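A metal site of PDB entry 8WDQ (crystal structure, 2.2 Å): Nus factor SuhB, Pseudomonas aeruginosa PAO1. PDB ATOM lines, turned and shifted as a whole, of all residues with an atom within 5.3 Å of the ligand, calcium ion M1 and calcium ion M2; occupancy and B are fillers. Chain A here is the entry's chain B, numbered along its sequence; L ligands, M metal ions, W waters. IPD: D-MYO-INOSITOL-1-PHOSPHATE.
Within 4 Å of calcium ion M2: Glu 69, Asp 88 and Leu 90.
Water W1 lies within hydrogen-bond range of the indole nitrogen of Trp 217 (3.2 Å) and the side-chain carboxylate of Glu 69 (3.3 Å).
Water W2 bridges OD1 of Asp 46 and OE2 of Glu 70.
Water W7 lies within hydrogen-bond range of the side-chain carboxylate of Glu 69, an oxygen (O7) of the ligand and the side-chain hydroxyl of Thr 93.
Water W8 lies within hydrogen-bond range of an oxygen (O8) of the ligand (2.6 Å), the backbone NH of Thr 94 (2.9 Å) and the backbone NH of Thr 93 (3.1 Å).
Water W6 bridges the side-chain carboxylate of Asp 218 and an oxygen (O2) of the ligand.
Water W4 lies within hydrogen-bond range of the side-chain carboxylate (OE1) of Glu 211 (2.6 Å), the side-chain carboxylate (OD2) of Asp 197 (3.0 Å), an oxygen (O5) of the ligand (3.0 Å), the guanidinium group (NH1) of Arg 190 (3.2 Å) and the backbone NH (N) of Ala 194 (3.4 Å).
An oxygen (O3) of the ligand sits at hydrogen-bond distance from the guanidinium group (NH2) of Arg 164, at 2.5 Å.
The backbone NH of Ala 194 is in hydrogen-bond range of an oxygen (O6) of the ligand.
An oxygen (O8) of the ligand lies within hydrogen-bond range of the backbone NH (N) of Gly 92.
The side-chain carboxylate of Glu 211 lies within hydrogen-bond range of an oxygen (O4) of the ligand (2.5 Å).
NH2 of Arg 190 lies within hydrogen-bond range of O4 of the ligand (2.8 Å).
An oxygen (O8) of the ligand lies within hydrogen-bond range of the backbone NH of Thr 93, 2.8 Å away.
The backbone NH (N) of Ala 193 sits at hydrogen-bond distance from an oxygen (O5) of the ligand.
OG1 of Thr 93 is in hydrogen-bond range of O8 of the ligand (3.2 Å).
O of Gly 192 sits close to O5 of the ligand, 3.0 Å away.
Merely in contact with the ligand: Phe 163 and Leu 214.
Within 4 Å of the ligand: Asp 88, Leu 90, Asp 91, Gly 92, Thr 93, Phe 163, Arg 164, Arg 190, Gly 192, Ala 193, Ala 194, Glu 211, Leu 214 and Asp 218.
Calcium ion M2 is bound by O9 of the ligand (2.3 Å), OD1 of Asp 88 (2.4 Å), O of Leu 90 (2.4 Å), OE1 of Glu 69 (2.4 Å), water W2 (2.5 Å), water W7 (2.5 Å) and OD2 of Asp 88 (2.6 Å).
Calcium ion M2 has seven donor atoms within binding distance.
Calcium ion M1 is bound by OD2 of Asp 88, OD1 of Asp 218, OD1 of Asp 91, O9 of the ligand and O1 of the ligand.
Slightly farther from calcium ion M1 lies water W1 (3.0 Å).
O of Gly 213 lies within hydrogen-bond range of NH2 of Arg 164.
OD2 of Asp 91 sits at hydrogen-bond distance from OG of Ser 195 (2.6 Å).
The backbone NH (N) of Ala 194 is in hydrogen-bond range of the side-chain carboxylate (OD2) of Asp 91, at 3.2 Å.
NE1 of Trp 217 lies close to OE1 of Glu 69.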
ATOM      1  N   ASP A  46     -18.373  20.711  26.664  1.00  0.00           N
ATOM      2  CA  ASP A  46     -17.610  20.808  25.428  1.00  0.00           C
ATOM      3  C   ASP A  46     -18.159  21.907  24.517  1.00  0.00           C
ATOM      4  O   ASP A  46     -17.420  22.773  24.036  1.00  0.00           O
ATOM      5  CB  ASP A  46     -17.658  19.473  24.679  1.00  0.00           C
ATOM      6  CG  ASP A  46     -16.621  18.476  25.158  1.00  0.00           C
ATOM      7  OD1 ASP A  46     -15.699  18.851  25.912  1.00  0.00           O
ATOM      8  OD2 ASP A  46     -16.730  17.292  24.758  1.00  0.00           O
ATOM      9  N   GLU A  69     -13.351  20.528  17.572  1.00  0.00           N
ATOM     10  CA  GLU A  69     -13.683  19.123  17.752  1.00  0.00           C
ATOM     11  C   GLU A  69     -15.199  18.917  17.722  1.00  0.00           C
ATOM     12  O   GLU A  69     -15.702  18.014  17.043  1.00  0.00           O
ATOM     13  CB  GLU A  69     -13.106  18.592  19.072  1.00  0.00           C
ATOM     14  CG  GLU A  69     -13.309  17.091  19.227  1.00  0.00           C
ATOM     15  CD  GLU A  69     -12.865  16.543  20.577  1.00  0.00           C
ATOM     16  OE1 GLU A  69     -12.138  17.248  21.319  1.00  0.00           O
ATOM     17  OE2 GLU A  69     -13.254  15.397  20.892  1.00  0.00           O
ATOM     18  N   GLU A  70     -15.935  19.771  18.429  1.00  0.00           N
ATOM     19  CA  GLU A  70     -17.393  19.640  18.469  1.00  0.00           C
ATOM     20  C   GLU A  70     -18.029  19.999  17.134  1.00  0.00           C
ATOM     21  O   GLU A  70     -18.933  19.297  16.666  1.00  0.00           O
ATOM     22  CB  GLU A  70     -17.971  20.518  19.583  1.00  0.00           C
ATOM     23  CG  GLU A  70     -17.538  20.193  21.030  1.00  0.00           C
ATOM     24  CD  GLU A  70     -17.045  18.761  21.219  1.00  0.00           C
ATOM     25  OE1 GLU A  70     -17.900  17.846  21.226  1.00  0.00           O
ATOM     26  OE2 GLU A  70     -15.813  18.556  21.409  1.00  0.00           O
ATOM     27  N   ASP A  88      -9.413  22.353  20.520  1.00  0.00           N
ATOM     28  CA  ASP A  88     -10.051  21.420  21.445  1.00  0.00           C
ATOM     29  C   ASP A  88     -10.543  22.206  22.641  1.00  0.00           C
ATOM     30  O   ASP A  88      -9.730  22.680  23.457  1.00  0.00           O
ATOM     31  CB  ASP A  88      -9.111  20.299  21.892  1.00  0.00           C
ATOM     32  CG  ASP A  88      -9.858  19.222  22.687  1.00  0.00           C
ATOM     33  OD1 ASP A  88     -11.014  19.458  23.074  1.00  0.00           O
ATOM     34  OD2 ASP A  88      -9.306  18.129  22.922  1.00  0.00           O
ATOM     35  N   PRO A  89     -11.858  22.354  22.808  1.00  0.00           N
ATOM     36  CA  PRO A  89     -12.375  23.154  23.913  1.00  0.00           C
ATOM     37  C   PRO A  89     -12.178  22.512  25.271  1.00  0.00           C
ATOM     38  O   PRO A  89     -12.214  23.221  26.286  1.00  0.00           O
ATOM     39  CB  PRO A  89     -13.872  23.287  23.574  1.00  0.00           C
ATOM     40  CG  PRO A  89     -14.174  22.073  22.779  1.00  0.00           C
ATOM     41  CD  PRO A  89     -12.930  21.720  22.018  1.00  0.00           C
ATOM     42  N   LEU A  90     -11.967  21.195  25.330  1.00  0.00           N
ATOM     43  CA  LEU A  90     -11.729  20.501  26.597  1.00  0.00           C
ATOM     44  C   LEU A  90     -10.925  19.245  26.306  1.00  0.00           C
ATOM     45  O   LEU A  90     -11.481  18.222  25.894  1.00  0.00           O
ATOM     46  CB  LEU A  90     -13.041  20.175  27.305  1.00  0.00           C
ATOM     47  CG  LEU A  90     -12.927  19.446  28.644  1.00  0.00           C
ATOM     48  CD1 LEU A  90     -11.842  20.041  29.507  1.00  0.00           C
ATOM     49  CD2 LEU A  90     -14.258  19.477  29.377  1.00  0.00           C
ATOM     50  N   ASP A  91      -9.618  19.334  26.530  1.00  0.00           N
ATOM     51  CA  ASP A  91      -8.712  18.190  26.398  1.00  0.00           C
ATOM     52  C   ASP A  91      -8.574  17.508  27.752  1.00  0.00           C
ATOM     53  O   ASP A  91      -8.141  18.142  28.722  1.00  0.00           O
ATOM     54  CB  ASP A  91      -7.344  18.665  25.890  1.00  0.00           C
ATOM     55  CG  ASP A  91      -6.389  17.520  25.631  1.00  0.00           C
ATOM     56  OD1 ASP A  91      -6.839  16.460  25.155  1.00  0.00           O
ATOM     57  OD2 ASP A  91      -5.186  17.673  25.910  1.00  0.00           O
ATOM     58  N   GLY A  92      -8.943  16.236  27.818  1.00  0.00           N
ATOM     59  CA  GLY A  92      -8.972  15.517  29.074  1.00  0.00           C
ATOM     60  C   GLY A  92     -10.384  15.334  29.601  1.00  0.00           C
ATOM     61  O   GLY A  92     -10.642  15.592  30.789  1.00  0.00           O
ATOM     62  N   THR A  93     -11.314  14.885  28.749  1.00  0.00           N
ATOM     63  CA  THR A  93     -12.717  14.818  29.150  1.00  0.00           C
ATOM     64  C   THR A  93     -13.019  13.664  30.082  1.00  0.00           C
ATOM     65  O   THR A  93     -13.940  13.770  30.899  1.00  0.00           O
ATOM     66  CB  THR A  93     -13.640  14.709  27.928  1.00  0.00           C
ATOM     67  OG1 THR A  93     -13.104  13.749  27.006  1.00  0.00           O
ATOM     68  CG2 THR A  93     -13.811  16.058  27.241  1.00  0.00           C
ATOM     69  N   THR A  94     -12.298  12.544  29.971  1.00  0.00           N
ATOM     70  CA  THR A  94     -12.510  11.440  30.904  1.00  0.00           C
ATOM     71  C   THR A  94     -12.113  11.844  32.319  1.00  0.00           C
ATOM     72  O   THR A  94     -12.862  11.627  33.292  1.00  0.00           O
ATOM     73  CB  THR A  94     -11.748  10.220  30.432  1.00  0.00           C
ATOM     74  OG1 THR A  94     -12.274   9.788  29.173  1.00  0.00           O
ATOM     75  CG2 THR A  94     -11.859   9.077  31.421  1.00  0.00           C
ATOM     76  N   GLY A 160       0.493   8.422  26.268  1.00  0.00           N
ATOM     77  CA  GLY A 160      -0.930   8.156  26.289  1.00  0.00           C
ATOM     78  C   GLY A 160      -1.201   6.707  25.961  1.00  0.00           C
ATOM     79  O   GLY A 160      -0.673   6.188  24.972  1.00  0.00           O
ATOM     80  N   PHE A 161      -1.985   6.023  26.797  1.00  0.00           N
ATOM     81  CA  PHE A 161      -2.281   4.622  26.577  1.00  0.00           C
ATOM     82  C   PHE A 161      -3.231   4.461  25.387  1.00  0.00           C
ATOM     83  O   PHE A 161      -4.120   5.290  25.179  1.00  0.00           O
ATOM     84  CB  PHE A 161      -2.927   4.003  27.811  1.00  0.00           C
ATOM     85  CG  PHE A 161      -2.075   4.054  29.041  1.00  0.00           C
ATOM     86  CD1 PHE A 161      -0.690   3.899  28.954  1.00  0.00           C
ATOM     87  CD2 PHE A 161      -2.649   4.247  30.282  1.00  0.00           C
ATOM     88  CE1 PHE A 161       0.087   3.950  30.082  1.00  0.00           C
ATOM     89  CE2 PHE A 161      -1.865   4.292  31.426  1.00  0.00           C
ATOM     90  CZ  PHE A 161      -0.496   4.133  31.324  1.00  0.00           C
ATOM     91  N   PHE A 163      -6.205   3.214  24.507  1.00  0.00           N
ATOM     92  CA  PHE A 163      -7.386   2.741  25.230  1.00  0.00           C
ATOM     93  C   PHE A 163      -8.576   2.437  24.344  1.00  0.00           C
ATOM     94  O   PHE A 163      -9.522   1.784  24.807  1.00  0.00           O
ATOM     95  CB  PHE A 163      -7.800   3.783  26.285  1.00  0.00           C
ATOM     96  CG  PHE A 163      -8.239   5.102  25.699  1.00  0.00           C
ATOM     97  CD1 PHE A 163      -7.313   6.077  25.373  1.00  0.00           C
ATOM     98  CD2 PHE A 163      -9.583   5.366  25.485  1.00  0.00           C
ATOM     99  CE1 PHE A 163      -7.725   7.290  24.821  1.00  0.00           C
ATOM    100  CE2 PHE A 163      -9.998   6.573  24.945  1.00  0.00           C
ATOM    101  CZ  PHE A 163      -9.069   7.535  24.613  1.00  0.00           C
ATOM    102  N   ARG A 164      -8.581   2.873  23.086  1.00  0.00           N
ATOM    103  CA  ARG A 164      -9.743   2.691  22.221  1.00  0.00           C
ATOM    104  C   ARG A 164      -9.836   1.260  21.713  1.00  0.00           C
ATOM    105  O   ARG A 164      -8.836   0.550  21.595  1.00  0.00           O
ATOM    106  CB  ARG A 164      -9.682   3.638  21.018  1.00  0.00           C
ATOM    107  CG  ARG A 164      -9.716   5.120  21.347  1.00  0.00           C
ATOM    108  CD  ARG A 164      -9.261   5.938  20.149  1.00  0.00           C
ATOM    109  NE  ARG A 164      -9.057   7.345  20.502  1.00  0.00           N
ATOM    110  CZ  ARG A 164      -7.944   7.814  21.052  1.00  0.00           C
ATOM    111  NH1 ARG A 164      -6.917   7.028  21.312  1.00  0.00           N
ATOM    112  NH2 ARG A 164      -7.873   9.111  21.346  1.00  0.00           N
ATOM    113  N   ARG A 190       1.225   8.858  32.656  1.00  0.00           N
ATOM    114  CA  ARG A 190       0.027   8.941  31.822  1.00  0.00           C
ATOM    115  C   ARG A 190      -1.028   9.705  32.633  1.00  0.00           C
ATOM    116  O   ARG A 190      -1.793   9.111  33.389  1.00  0.00           O
ATOM    117  CB  ARG A 190      -0.461   7.554  31.403  1.00  0.00           C
ATOM    118  CG  ARG A 190      -1.352   7.561  30.152  1.00  0.00           C
ATOM    119  CD  ARG A 190      -2.801   7.915  30.481  1.00  0.00           C
ATOM    120  NE  ARG A 190      -3.743   7.630  29.391  1.00  0.00           N
ATOM    121  CZ  ARG A 190      -4.003   8.453  28.382  1.00  0.00           C
ATOM    122  NH1 ARG A 190      -3.395   9.627  28.271  1.00  0.00           N
ATOM    123  NH2 ARG A 190      -4.886   8.084  27.462  1.00  0.00           N
ATOM    124  N   GLY A 192      -3.382  12.034  31.314  1.00  0.00           N
ATOM    125  CA  GLY A 192      -4.684  12.057  30.666  1.00  0.00           C
ATOM    126  C   GLY A 192      -5.070  13.297  29.881  1.00  0.00           C
ATOM    127  O   GLY A 192      -6.257  13.506  29.648  1.00  0.00           O
ATOM    128  N   ALA A 193      -4.108  14.113  29.433  1.00  0.00           N
ATOM    129  CA  ALA A 193      -4.437  15.215  28.526  1.00  0.00           C
ATOM    130  C   ALA A 193      -3.217  15.467  27.648  1.00  0.00           C
ATOM    131  O   ALA A 193      -2.192  15.952  28.142  1.00  0.00           O
ATOM    132  CB  ALA A 193      -4.852  16.469  29.297  1.00  0.00           C
ATOM    133  N   ALA A 194      -3.333  15.138  26.364  1.00  0.00           N
ATOM    134  CA  ALA A 194      -2.161  15.150  25.488  1.00  0.00           C
ATOM    135  C   ALA A 194      -1.630  16.556  25.273  1.00  0.00           C
ATOM    136  O   ALA A 194      -0.421  16.751  25.108  1.00  0.00           O
ATOM    137  CB  ALA A 194      -2.492  14.494  24.148  1.00  0.00           C
ATOM    138  N   SER A 195      -2.522  17.552  25.249  1.00  0.00           N
ATOM    139  CA  SER A 195      -2.054  18.924  25.114  1.00  0.00           C
ATOM    140  C   SER A 195      -1.164  19.312  26.284  1.00  0.00           C
ATOM    141  O   SER A 195      -0.123  19.959  26.097  1.00  0.00           O
ATOM    142  CB  SER A 195      -3.244  19.882  24.975  1.00  0.00           C
ATOM    143  OG  SER A 195      -3.986  19.992  26.169  1.00  0.00           O
ATOM    144  N   ASP A 197       0.568  17.113  28.077  1.00  0.00           N
ATOM    145  CA  ASP A 197       1.790  16.333  27.933  1.00  0.00           C
ATOM    146  C   ASP A 197       2.786  17.034  27.015  1.00  0.00           C
ATOM    147  O   ASP A 197       3.990  17.117  27.308  1.00  0.00           O
ATOM    148  CB  ASP A 197       1.483  14.933  27.400  1.00  0.00           C
ATOM    149  CG  ASP A 197       0.685  14.089  28.386  1.00  0.00           C
ATOM    150  OD1 ASP A 197       0.940  14.181  29.608  1.00  0.00           O
ATOM    151  OD2 ASP A 197      -0.210  13.331  27.939  1.00  0.00           O
ATOM    152  N   GLU A 211       2.668   9.025  21.584  1.00  0.00           N
ATOM    153  CA  GLU A 211       1.299   8.527  21.613  1.00  0.00           C
ATOM    154  C   GLU A 211       0.819   8.353  20.181  1.00  0.00           C
ATOM    155  O   GLU A 211       1.274   9.061  19.287  1.00  0.00           O
ATOM    156  CB  GLU A 211       0.368   9.485  22.387  1.00  0.00           C
ATOM    157  CG  GLU A 211      -1.108   9.092  22.369  1.00  0.00           C
ATOM    158  CD  GLU A 211      -1.956   9.798  23.411  1.00  0.00           C
ATOM    159  OE1 GLU A 211      -1.501  10.805  23.984  1.00  0.00           O
ATOM    160  OE2 GLU A 211      -3.083   9.337  23.672  1.00  0.00           O
ATOM    161  N   GLY A 213      -3.025   7.494  17.836  1.00  0.00           N
ATOM    162  CA  GLY A 213      -4.465   7.624  17.903  1.00  0.00           C
ATOM    163  C   GLY A 213      -4.986   9.016  18.161  1.00  0.00           C
ATOM    164  O   GLY A 213      -6.188   9.184  18.402  1.00  0.00           O
ATOM    165  N   LEU A 214      -4.120  10.039  18.130  1.00  0.00           N
ATOM    166  CA  LEU A 214      -4.552  11.396  18.451  1.00  0.00           C
ATOM    167  C   LEU A 214      -5.172  12.081  17.241  1.00  0.00           C
ATOM    168  O   LEU A 214      -5.010  11.660  16.089  1.00  0.00           O
ATOM    169  CB  LEU A 214      -3.376  12.229  18.962  1.00  0.00           C
ATOM    170  CG  LEU A 214      -2.813  11.923  20.355  1.00  0.00           C
ATOM    171  CD1 LEU A 214      -1.539  12.701  20.618  1.00  0.00           C
ATOM    172  CD2 LEU A 214      -3.853  12.232  21.418  1.00  0.00           C
ATOM    173  N   TRP A 217      -6.581  18.488  16.873  1.00  0.00           N
ATOM    174  CA  TRP A 217      -6.795  19.445  17.945  1.00  0.00           C
ATOM    175  C   TRP A 217      -6.102  19.037  19.238  1.00  0.00           C
ATOM    176  O   TRP A 217      -5.832  19.898  20.078  1.00  0.00           O
ATOM    177  CB  TRP A 217      -8.286  19.678  18.192  1.00  0.00           C
ATOM    178  CG  TRP A 217      -9.112  18.443  18.065  1.00  0.00           C
ATOM    179  CD1 TRP A 217      -9.310  17.485  19.029  1.00  0.00           C
ATOM    180  CD2 TRP A 217      -9.873  18.028  16.924  1.00  0.00           C
ATOM    181  NE1 TRP A 217     -10.140  16.502  18.548  1.00  0.00           N
ATOM    182  CE2 TRP A 217     -10.496  16.815  17.264  1.00  0.00           C
ATOM    183  CE3 TRP A 217     -10.070  18.573  15.655  1.00  0.00           C
ATOM    184  CZ2 TRP A 217     -11.312  16.125  16.366  1.00  0.00           C
ATOM    185  CZ3 TRP A 217     -10.889  17.895  14.763  1.00  0.00           C
ATOM    186  CH2 TRP A 217     -11.499  16.679  15.130  1.00  0.00           C
ATOM    187  N   ASP A 218      -5.790  17.743  19.409  1.00  0.00           N
ATOM    188  CA  ASP A 218      -5.001  17.317  20.562  1.00  0.00           C
ATOM    189  C   ASP A 218      -3.565  17.837  20.480  1.00  0.00           C
ATOM    190  O   ASP A 218      -2.965  18.159  21.513  1.00  0.00           O
ATOM    191  CB  ASP A 218      -4.947  15.789  20.666  1.00  0.00           C
ATOM    192  CG  ASP A 218      -6.311  15.159  20.776  1.00  0.00           C
ATOM    193  OD1 ASP A 218      -7.217  15.780  21.365  1.00  0.00           O
ATOM    194  OD2 ASP A 218      -6.464  14.025  20.267  1.00  0.00           O
HETATM  195  C1  IPD L   1      -7.649  12.814  24.916  1.00  0.00           C
HETATM  196  C2  IPD L   1      -7.239  12.057  23.640  1.00  0.00           C
HETATM  197  C3  IPD L   1      -6.102  11.033  23.862  1.00  0.00           C
HETATM  198  C4  IPD L   1      -5.750  10.859  25.340  1.00  0.00           C
HETATM  199  C5  IPD L   1      -5.353  12.211  25.930  1.00  0.00           C
HETATM  200  C6  IPD L   1      -6.431  13.286  25.742  1.00  0.00           C
HETATM  201  P1  IPD L   1      -9.941  14.208  24.946  1.00  0.00           P
HETATM  202  O1  IPD L   1      -8.386  13.934  24.457  1.00  0.00           O
HETATM  203  O2  IPD L   1      -8.377  11.453  23.061  1.00  0.00           O
HETATM  204  O3  IPD L   1      -6.415   9.797  23.281  1.00  0.00           O
HETATM  205  O4  IPD L   1      -4.638  10.016  25.469  1.00  0.00           O
HETATM  206  O5  IPD L   1      -5.033  12.084  27.293  1.00  0.00           O
HETATM  207  O6  IPD L   1      -5.754  14.317  25.051  1.00  0.00           O
HETATM  208  O7  IPD L   1     -10.869  13.208  24.307  1.00  0.00           O
HETATM  209  O8  IPD L   1     -10.011  14.102  26.453  1.00  0.00           O
HETATM  210  O9  IPD L   1     -10.335  15.595  24.506  1.00  0.00           O
HETATM  211 CA    CA M   1      -8.285  16.173  23.307  1.00  0.00          CA
HETATM  212 CA    CA M   2     -11.646  17.269  23.715  1.00  0.00          CA
HETATM  213  O   HOH W   1     -10.026  14.811  21.271  1.00  0.00           O
HETATM  214  O   HOH W   2     -13.860  18.390  23.854  1.00  0.00           O
HETATM  215  O   HOH W   3     -10.675  10.459  24.755  1.00  0.00           O
HETATM  216  O   HOH W   4      -2.196  11.893  26.282  1.00  0.00           O
HETATM  217  O   HOH W   5     -11.374   9.940  22.454  1.00  0.00           O
HETATM  218  O   HOH W   6      -8.474  12.509  20.553  1.00  0.00           O
HETATM  219  O   HOH W   7     -13.093  15.246  23.905  1.00  0.00           O
HETATM  220  O   HOH W   8     -10.174  12.027  28.091  1.00  0.00           O
